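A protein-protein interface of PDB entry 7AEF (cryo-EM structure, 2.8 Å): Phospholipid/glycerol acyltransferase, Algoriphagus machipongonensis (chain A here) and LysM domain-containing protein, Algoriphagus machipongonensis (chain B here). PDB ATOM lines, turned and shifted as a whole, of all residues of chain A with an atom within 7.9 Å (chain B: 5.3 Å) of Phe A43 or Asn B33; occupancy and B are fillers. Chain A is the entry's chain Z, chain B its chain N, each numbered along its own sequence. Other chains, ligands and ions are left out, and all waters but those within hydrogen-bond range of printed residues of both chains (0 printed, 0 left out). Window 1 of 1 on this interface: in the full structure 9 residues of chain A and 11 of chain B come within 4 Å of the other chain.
N of Asn B33 lies within hydrogen-bond range of OE2 of Glu A45 (3.3 Å). ND2 of Asn B33 sits close to O of Gly A46 (3.5 Å). The backbone carbonyl oxygen (O) of Pro B34 sits at hydrogen-bond distance from the backbone NH (N) of Gly A46 (3.0 Å).
Of chain B, only Asn B33 (3.7 Å) comes within 4 Å of Phe A43. Printed residues of chain B within 4 Å of Gly A46: Asn B33, Pro B34 and Trp B118. Glu B7 touches none of the printed residues of chain A. Of the printed residues of chain A, Lys B8 touches Glu A45 (3.2 Å). Of chain A, only Phe A43, Glu A45 and Gly A46 come within 4 Å of Asn B33. Pro B34 touches one residue of chain A. Printed residues of chain A within 4 Å of Trp B118: Gly A46. Met B147 touches none of the printed residues of chain A. The nearest printed residue of chain A that does not touch Glu B35 is Gly A46 (4.004 Å).
Of the 13 printed residues of chain A, 5 touch a printed residue of chain B. Hydrophobic or aromatic side chains of chain A within 4 Å of the printed part of chain B: Phe A43. Hydrophobic or aromatic side chains of chain B that line the printed part of chain A: Leu B6, Leu B32 and Trp B118. Among the printed residues, 9 pairs touch across the chains. Among the printed residues, no Asp or Glu carboxylate lies within 4 Å of a Lys or Arg side-chain nitrogen of the other chain.
The backbone carbonyl oxygen (O) of Glu B7 lies within hydrogen-bond range of the side-chain amide nitrogen (ND2) of Asn B33 (2.9 Å). NE1 of Trp B118 sits at hydrogen-bond distance from O of Glu B7 (3.3 Å). The backbone NH of Leu B9 is in hydrogen-bond range of the side-chain amide oxygen of Asn B33 (3.2 Å). OG1 of Thr B30 is in hydrogen-bond range of O of Leu B32 (3.0 Å). The backbone carbonyl oxygen (O) of Phe A43 sits at hydrogen-bond distance from the backbone NH (N) of His A53, 2.9 Å away. The side-chain carboxylate of Glu A45 is in hydrogen-bond range of a ring nitrogen (NE2) of His A53 (2.9 Å).
CZ of Phe A43 touches O of Asn B33, at 3.7 Å. Glu B35 touches Ala A44 (CB to O, 3.6 Å). Lys B8 touches Glu A45. OE2 of Glu A45 touches CA of Leu B32, at 3.6 Å. Trp B118 touches Gly A46 (CZ2 to O, 3.8 Å). Gly A47 touches Leu B6 (O to CD1, 3.5 Å).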
ATOM      1  N   GLU A  41     -17.146  19.602 -28.153  1.00  0.00           N
ATOM      2  CA  GLU A  41     -17.725  19.027 -26.935  1.00  0.00           C
ATOM      3  C   GLU A  41     -18.638  19.973 -26.192  1.00  0.00           C
ATOM      4  O   GLU A  41     -18.457  21.180 -26.246  1.00  0.00           O
ATOM      5  CB  GLU A  41     -16.695  18.486 -25.953  1.00  0.00           C
ATOM      6  CG  GLU A  41     -15.809  17.427 -26.471  1.00  0.00           C
ATOM      7  CD  GLU A  41     -14.764  17.030 -25.474  1.00  0.00           C
ATOM      8  OE1 GLU A  41     -14.609  17.740 -24.482  1.00  0.00           O
ATOM      9  OE2 GLU A  41     -14.093  16.014 -25.678  1.00  0.00           O
ATOM     10  N   GLU A  42     -19.612  19.418 -25.470  1.00  0.00           N
ATOM     11  CA  GLU A  42     -20.567  20.239 -24.738  1.00  0.00           C
ATOM     12  C   GLU A  42     -20.389  20.168 -23.221  1.00  0.00           C
ATOM     13  O   GLU A  42     -19.965  19.149 -22.676  1.00  0.00           O
ATOM     14  CB  GLU A  42     -21.989  19.813 -25.071  1.00  0.00           C
ATOM     15  CG  GLU A  42     -22.417  20.163 -26.474  1.00  0.00           C
ATOM     16  CD  GLU A  42     -23.819  19.704 -26.806  1.00  0.00           C
ATOM     17  OE1 GLU A  42     -24.583  19.353 -25.898  1.00  0.00           O
ATOM     18  OE2 GLU A  42     -24.242  19.941 -27.947  1.00  0.00           O
ATOM     19  N   PHE A  43     -20.784  21.253 -22.541  1.00  0.00           N
ATOM     20  CA  PHE A  43     -20.758  21.326 -21.081  1.00  0.00           C
ATOM     21  C   PHE A  43     -21.888  22.176 -20.499  1.00  0.00           C
ATOM     22  O   PHE A  43     -22.140  23.296 -20.949  1.00  0.00           O
ATOM     23  CB  PHE A  43     -19.422  21.882 -20.619  1.00  0.00           C
ATOM     24  CG  PHE A  43     -19.334  22.076 -19.163  1.00  0.00           C
ATOM     25  CD1 PHE A  43     -19.129  21.012 -18.320  1.00  0.00           C
ATOM     26  CD2 PHE A  43     -19.444  23.340 -18.629  1.00  0.00           C
ATOM     27  CE1 PHE A  43     -19.053  21.211 -16.966  1.00  0.00           C
ATOM     28  CE2 PHE A  43     -19.374  23.541 -17.291  1.00  0.00           C
ATOM     29  CZ  PHE A  43     -19.178  22.477 -16.454  1.00  0.00           C
ATOM     30  N   ALA A  44     -22.531  21.673 -19.457  1.00  0.00           N
ATOM     31  CA  ALA A  44     -23.580  22.424 -18.781  1.00  0.00           C
ATOM     32  C   ALA A  44     -23.057  23.031 -17.490  1.00  0.00           C
ATOM     33  O   ALA A  44     -22.605  22.310 -16.599  1.00  0.00           O
ATOM     34  CB  ALA A  44     -24.774  21.533 -18.483  1.00  0.00           C
ATOM     35  N   GLU A  45     -23.155  24.343 -17.375  1.00  0.00           N
ATOM     36  CA  GLU A  45     -22.704  25.057 -16.191  1.00  0.00           C
ATOM     37  C   GLU A  45     -23.879  25.292 -15.256  1.00  0.00           C
ATOM     38  O   GLU A  45     -24.899  25.837 -15.680  1.00  0.00           O
ATOM     39  CB  GLU A  45     -22.079  26.387 -16.596  1.00  0.00           C
ATOM     40  CG  GLU A  45     -21.548  27.164 -15.442  1.00  0.00           C
ATOM     41  CD  GLU A  45     -20.955  28.470 -15.835  1.00  0.00           C
ATOM     42  OE1 GLU A  45     -21.019  28.844 -17.010  1.00  0.00           O
ATOM     43  OE2 GLU A  45     -20.403  29.128 -14.959  1.00  0.00           O
ATOM     44  N   GLY A  46     -23.751  24.882 -14.000  1.00  0.00           N
ATOM     45  CA  GLY A  46     -24.850  25.095 -13.083  1.00  0.00           C
ATOM     46  C   GLY A  46     -25.167  26.564 -12.897  1.00  0.00           C
ATOM     47  O   GLY A  46     -24.269  27.375 -12.694  1.00  0.00           O
ATOM     48  N   GLY A  47     -26.444  26.919 -13.000  1.00  0.00           N
ATOM     49  CA  GLY A  47     -26.902  28.285 -12.889  1.00  0.00           C
ATOM     50  C   GLY A  47     -27.093  28.991 -14.214  1.00  0.00           C
ATOM     51  O   GLY A  47     -27.736  30.037 -14.266  1.00  0.00           O
ATOM     52  N   GLU A  48     -26.551  28.463 -15.272  1.00  0.00           N
ATOM     53  CA  GLU A  48     -26.698  29.057 -16.579  1.00  0.00           C
ATOM     54  C   GLU A  48     -27.740  28.234 -17.329  1.00  0.00           C
ATOM     55  O   GLU A  48     -27.443  27.137 -17.779  1.00  0.00           O
ATOM     56  CB  GLU A  48     -25.329  29.040 -17.245  1.00  0.00           C
ATOM     57  CG  GLU A  48     -25.306  29.285 -18.728  1.00  0.00           C
ATOM     58  CD  GLU A  48     -25.492  30.729 -19.079  1.00  0.00           C
ATOM     59  OE1 GLU A  48     -24.533  31.513 -18.931  1.00  0.00           O
ATOM     60  OE2 GLU A  48     -26.610  31.086 -19.479  1.00  0.00           O
ATOM     61  N   PHE A  51     -28.213  28.347 -22.281  1.00  0.00           N
ATOM     62  CA  PHE A  51     -27.518  27.586 -23.316  1.00  0.00           C
ATOM     63  C   PHE A  51     -26.473  26.681 -22.679  1.00  0.00           C
ATOM     64  O   PHE A  51     -26.072  26.879 -21.534  1.00  0.00           O
ATOM     65  CB  PHE A  51     -26.853  28.506 -24.351  1.00  0.00           C
ATOM     66  CG  PHE A  51     -25.951  29.540 -23.763  1.00  0.00           C
ATOM     67  CD1 PHE A  51     -24.622  29.265 -23.530  1.00  0.00           C
ATOM     68  CD2 PHE A  51     -26.427  30.793 -23.465  1.00  0.00           C
ATOM     69  CE1 PHE A  51     -23.809  30.196 -22.990  1.00  0.00           C
ATOM     70  CE2 PHE A  51     -25.611  31.732 -22.923  1.00  0.00           C
ATOM     71  CZ  PHE A  51     -24.301  31.435 -22.685  1.00  0.00           C
ATOM     72  N   LYS A  52     -25.986  25.722 -23.453  1.00  0.00           N
ATOM     73  CA  LYS A  52     -24.834  24.941 -23.025  1.00  0.00           C
ATOM     74  C   LYS A  52     -23.594  25.509 -23.684  1.00  0.00           C
ATOM     75  O   LYS A  52     -23.677  26.153 -24.723  1.00  0.00           O
ATOM     76  CB  LYS A  52     -24.987  23.467 -23.388  1.00  0.00           C
ATOM     77  CG  LYS A  52     -26.128  22.779 -22.700  1.00  0.00           C
ATOM     78  CD  LYS A  52     -26.290  21.352 -23.187  1.00  0.00           C
ATOM     79  CE  LYS A  52     -25.241  20.411 -22.612  1.00  0.00           C
ATOM     80  NZ  LYS A  52     -25.407  19.032 -23.142  1.00  0.00           N
ATOM     81  N   HIS A  53     -22.444  25.274 -23.076  1.00  0.00           N
ATOM     82  CA  HIS A  53     -21.197  25.740 -23.650  1.00  0.00           C
ATOM     83  C   HIS A  53     -20.694  24.730 -24.660  1.00  0.00           C
ATOM     84  O   HIS A  53     -20.910  23.532 -24.509  1.00  0.00           O
ATOM     85  CB  HIS A  53     -20.141  25.922 -22.577  1.00  0.00           C
ATOM     86  CG  HIS A  53     -20.467  26.973 -21.578  1.00  0.00           C
ATOM     87  ND1 HIS A  53     -20.453  28.315 -21.874  1.00  0.00           N
ATOM     88  CD2 HIS A  53     -20.795  26.876 -20.272  1.00  0.00           C
ATOM     89  CE1 HIS A  53     -20.761  29.002 -20.789  1.00  0.00           C
ATOM     90  NE2 HIS A  53     -20.970  28.152 -19.804  1.00  0.00           N
ATOM     91  N   LYS A  54     -19.994  25.210 -25.677  1.00  0.00           N
ATOM     92  CA  LYS A  54     -19.412  24.330 -26.676  1.00  0.00           C
ATOM     93  C   LYS A  54     -17.945  24.657 -26.855  1.00  0.00           C
ATOM     94  O   LYS A  54     -17.573  25.825 -26.911  1.00  0.00           O
ATOM     95  CB  LYS A  54     -20.133  24.468 -28.004  1.00  0.00           C
ATOM     96  CG  LYS A  54     -21.569  24.099 -27.902  1.00  0.00           C
ATOM     97  CD  LYS A  54     -22.289  24.195 -29.200  1.00  0.00           C
ATOM     98  CE  LYS A  54     -23.758  23.859 -28.998  1.00  0.00           C
ATOM     99  NZ  LYS A  54     -24.533  23.957 -30.263  1.00  0.00           N
ATOM    100  N   PHE A  55     -17.122  23.630 -26.986  1.00  0.00           N
ATOM    101  CA  PHE A  55     -15.693  23.830 -27.112  1.00  0.00           C
ATOM    102  C   PHE A  55     -15.158  23.062 -28.302  1.00  0.00           C
ATOM    103  O   PHE A  55     -15.552  21.939 -28.485  1.00  0.00           O
ATOM    104  CB  PHE A  55     -14.978  23.324 -25.881  1.00  0.00           C
ATOM    105  CG  PHE A  55     -15.503  23.883 -24.654  1.00  0.00           C
ATOM    106  CD1 PHE A  55     -16.481  23.214 -23.977  1.00  0.00           C
ATOM    107  CD2 PHE A  55     -15.051  25.085 -24.168  1.00  0.00           C
ATOM    108  CE1 PHE A  55     -17.008  23.716 -22.850  1.00  0.00           C
ATOM    109  CE2 PHE A  55     -15.578  25.596 -23.012  1.00  0.00           C
ATOM    110  CZ  PHE A  55     -16.560  24.907 -22.356  1.00  0.00           C
ATOM    111  N   LEU B   6     -24.944  36.006 -11.964  1.00  0.00           N
ATOM    112  CA  LEU B   6     -24.537  34.606 -11.885  1.00  0.00           C
ATOM    113  C   LEU B   6     -23.431  34.475 -10.845  1.00  0.00           C
ATOM    114  O   LEU B   6     -22.297  34.900 -11.077  1.00  0.00           O
ATOM    115  CB  LEU B   6     -24.074  34.101 -13.248  1.00  0.00           C
ATOM    116  CG  LEU B   6     -23.703  32.614 -13.351  1.00  0.00           C
ATOM    117  CD1 LEU B   6     -24.905  31.734 -13.118  1.00  0.00           C
ATOM    118  CD2 LEU B   6     -23.083  32.299 -14.691  1.00  0.00           C
ATOM    119  N   GLU B   7     -23.751  33.876  -9.705  1.00  0.00           N
ATOM    120  CA  GLU B   7     -22.773  33.692  -8.643  1.00  0.00           C
ATOM    121  C   GLU B   7     -21.854  32.515  -8.954  1.00  0.00           C
ATOM    122  O   GLU B   7     -22.272  31.517  -9.544  1.00  0.00           O
ATOM    123  CB  GLU B   7     -23.490  33.476  -7.307  1.00  0.00           C
ATOM    124  CG  GLU B   7     -22.593  33.531  -6.075  1.00  0.00           C
ATOM    125  CD  GLU B   7     -22.231  34.950  -5.655  1.00  0.00           C
ATOM    126  OE1 GLU B   7     -21.272  35.112  -4.878  1.00  0.00           O
ATOM    127  OE2 GLU B   7     -22.905  35.904  -6.090  1.00  0.00           O
ATOM    128  N   LYS B   8     -20.590  32.639  -8.558  1.00  0.00           N
ATOM    129  CA  LYS B   8     -19.566  31.632  -8.789  1.00  0.00           C
ATOM    130  C   LYS B   8     -19.125  31.017  -7.468  1.00  0.00           C
ATOM    131  O   LYS B   8     -19.096  31.692  -6.437  1.00  0.00           O
ATOM    132  CB  LYS B   8     -18.372  32.249  -9.513  1.00  0.00           C
ATOM    133  CG  LYS B   8     -18.649  32.568 -10.962  1.00  0.00           C
ATOM    134  CD  LYS B   8     -18.677  31.305 -11.789  1.00  0.00           C
ATOM    135  CE  LYS B   8     -19.402  31.521 -13.090  1.00  0.00           C
ATOM    136  NZ  LYS B   8     -18.830  32.650 -13.852  1.00  0.00           N
ATOM    137  N   LEU B   9     -18.777  29.733  -7.507  1.00  0.00           N
ATOM    138  CA  LEU B   9     -18.428  28.983  -6.304  1.00  0.00           C
ATOM    139  C   LEU B   9     -17.051  29.396  -5.786  1.00  0.00           C
ATOM    140  O   LEU B   9     -16.141  29.682  -6.564  1.00  0.00           O
ATOM    141  CB  LEU B   9     -18.491  27.484  -6.617  1.00  0.00           C
ATOM    142  CG  LEU B   9     -17.873  26.359  -5.783  1.00  0.00           C
ATOM    143  CD1 LEU B   9     -18.336  26.399  -4.373  1.00  0.00           C
ATOM    144  CD2 LEU B   9     -18.251  25.034  -6.365  1.00  0.00           C
ATOM    145  N   THR B  30     -13.796  29.832  -8.755  1.00  0.00           N
ATOM    146  CA  THR B  30     -13.855  29.112 -10.015  1.00  0.00           C
ATOM    147  C   THR B  30     -14.302  30.040 -11.149  1.00  0.00           C
ATOM    148  O   THR B  30     -14.848  31.123 -10.930  1.00  0.00           O
ATOM    149  CB  THR B  30     -14.786  27.900  -9.899  1.00  0.00           C
ATOM    150  OG1 THR B  30     -14.509  26.980 -10.956  1.00  0.00           O
ATOM    151  CG2 THR B  30     -16.242  28.309  -9.981  1.00  0.00           C
ATOM    152  N   LEU B  31     -14.034  29.612 -12.377  1.00  0.00           N
ATOM    153  CA  LEU B  31     -14.501  30.338 -13.548  1.00  0.00           C
ATOM    154  C   LEU B  31     -15.701  29.683 -14.211  1.00  0.00           C
ATOM    155  O   LEU B  31     -16.422  30.355 -14.951  1.00  0.00           O
ATOM    156  CB  LEU B  31     -13.374  30.485 -14.576  1.00  0.00           C
ATOM    157  CG  LEU B  31     -12.084  31.183 -14.131  1.00  0.00           C
ATOM    158  CD1 LEU B  31     -10.927  30.727 -14.985  1.00  0.00           C
ATOM    159  CD2 LEU B  31     -12.205  32.691 -14.181  1.00  0.00           C
ATOM    160  N   LEU B  32     -15.918  28.393 -13.974  1.00  0.00           N
ATOM    161  CA  LEU B  32     -17.117  27.694 -14.410  1.00  0.00           C
ATOM    162  C   LEU B  32     -17.645  26.861 -13.256  1.00  0.00           C
ATOM    163  O   LEU B  32     -16.893  26.129 -12.616  1.00  0.00           O
ATOM    164  CB  LEU B  32     -16.846  26.798 -15.618  1.00  0.00           C
ATOM    165  CG  LEU B  32     -16.375  27.470 -16.905  1.00  0.00           C
ATOM    166  CD1 LEU B  32     -15.589  26.485 -17.739  1.00  0.00           C
ATOM    167  CD2 LEU B  32     -17.550  28.022 -17.683  1.00  0.00           C
ATOM    168  N   ASN B  33     -18.922  26.979 -13.009  1.00  0.00           N
ATOM    169  CA  ASN B  33     -19.629  26.285 -11.946  1.00  0.00           C
ATOM    170  C   ASN B  33     -19.792  24.806 -12.280  1.00  0.00           C
ATOM    171  O   ASN B  33     -19.887  24.435 -13.451  1.00  0.00           O
ATOM    172  CB  ASN B  33     -21.012  26.907 -11.749  1.00  0.00           C
ATOM    173  CG  ASN B  33     -20.992  28.089 -10.816  1.00  0.00           C
ATOM    174  OD1 ASN B  33     -20.341  28.055  -9.785  1.00  0.00           O
ATOM    175  ND2 ASN B  33     -21.703  29.141 -11.174  1.00  0.00           N
ATOM    176  N   PRO B  34     -19.832  23.938 -11.270  1.00  0.00           N
ATOM    177  CA  PRO B  34     -20.220  22.547 -11.512  1.00  0.00           C
ATOM    178  C   PRO B  34     -21.678  22.452 -11.946  1.00  0.00           C
ATOM    179  O   PRO B  34     -22.465  23.381 -11.775  1.00  0.00           O
ATOM    180  CB  PRO B  34     -19.994  21.871 -10.157  1.00  0.00           C
ATOM    181  CG  PRO B  34     -19.100  22.769  -9.414  1.00  0.00           C
ATOM    182  CD  PRO B  34     -19.396  24.149  -9.881  1.00  0.00           C
ATOM    183  N   GLU B  35     -21.996  21.344 -12.609  1.00  0.00           N
ATOM    184  CA  GLU B  35     -23.368  21.021 -13.013  1.00  0.00           C
ATOM    185  C   GLU B  35     -24.303  20.659 -11.863  1.00  0.00           C
ATOM    186  O   GLU B  35     -25.484  21.036 -11.867  1.00  0.00           O
ATOM    187  CB  GLU B  35     -23.353  19.908 -14.060  1.00  0.00           C
ATOM    188  CG  GLU B  35     -24.731  19.531 -14.577  1.00  0.00           C
ATOM    189  CD  GLU B  35     -24.695  18.370 -15.547  1.00  0.00           C
ATOM    190  OE1 GLU B  35     -23.580  17.935 -15.911  1.00  0.00           O
ATOM    191  OE2 GLU B  35     -25.772  17.949 -16.017  1.00  0.00           O
ATOM    192  N   LEU B  73     -14.172  22.029 -14.293  1.00  0.00           N
ATOM    193  CA  LEU B  73     -13.571  22.135 -15.615  1.00  0.00           C
ATOM    194  C   LEU B  73     -12.765  23.424 -15.702  1.00  0.00           C
ATOM    195  O   LEU B  73     -13.256  24.493 -15.325  1.00  0.00           O
ATOM    196  CB  LEU B  73     -14.636  22.101 -16.712  1.00  0.00           C
ATOM    197  CG  LEU B  73     -14.154  22.238 -18.155  1.00  0.00           C
ATOM    198  CD1 LEU B  73     -13.566  20.941 -18.652  1.00  0.00           C
ATOM    199  CD2 LEU B  73     -15.279  22.688 -19.051  1.00  0.00           C
ATOM    200  N   TRP B 118     -21.530  28.388  -2.069  1.00  0.00           N
ATOM    201  CA  TRP B 118     -22.130  28.749  -3.352  1.00  0.00           C
ATOM    202  C   TRP B 118     -23.634  28.836  -3.161  1.00  0.00           C
ATOM    203  O   TRP B 118     -24.298  27.806  -3.046  1.00  0.00           O
ATOM    204  CB  TRP B 118     -21.784  27.730  -4.432  1.00  0.00           C
ATOM    205  CG  TRP B 118     -22.437  27.987  -5.758  1.00  0.00           C
ATOM    206  CD1 TRP B 118     -22.679  29.197  -6.331  1.00  0.00           C
ATOM    207  CD2 TRP B 118     -22.920  27.008  -6.677  1.00  0.00           C
ATOM    208  NE1 TRP B 118     -23.294  29.036  -7.540  1.00  0.00           N
ATOM    209  CE2 TRP B 118     -23.450  27.699  -7.779  1.00  0.00           C
ATOM    210  CE3 TRP B 118     -22.958  25.611  -6.675  1.00  0.00           C
ATOM    211  CZ2 TRP B 118     -24.018  27.043  -8.868  1.00  0.00           C
ATOM    212  CZ3 TRP B 118     -23.515  24.963  -7.760  1.00  0.00           C
ATOM    213  CH2 TRP B 118     -24.037  25.679  -8.841  1.00  0.00           C
ATOM    214  N   MET B 147      -9.787  18.535 -16.298  1.00  0.00           N
ATOM    215  CA  MET B 147     -10.993  18.119 -15.588  1.00  0.00           C
ATOM    216  C   MET B 147     -10.608  17.536 -14.232  1.00  0.00           C
ATOM    217  O   MET B 147      -9.664  16.750 -14.143  1.00  0.00           O
ATOM    218  CB  MET B 147     -11.751  17.073 -16.403  1.00  0.00           C
ATOM    219  CG  MET B 147     -13.172  16.792 -15.958  1.00  0.00           C
ATOM    220  SD  MET B 147     -14.329  18.098 -16.401  1.00  0.00           S
ATOM    221  CE  MET B 147     -15.639  17.844 -15.205  1.00  0.00           C
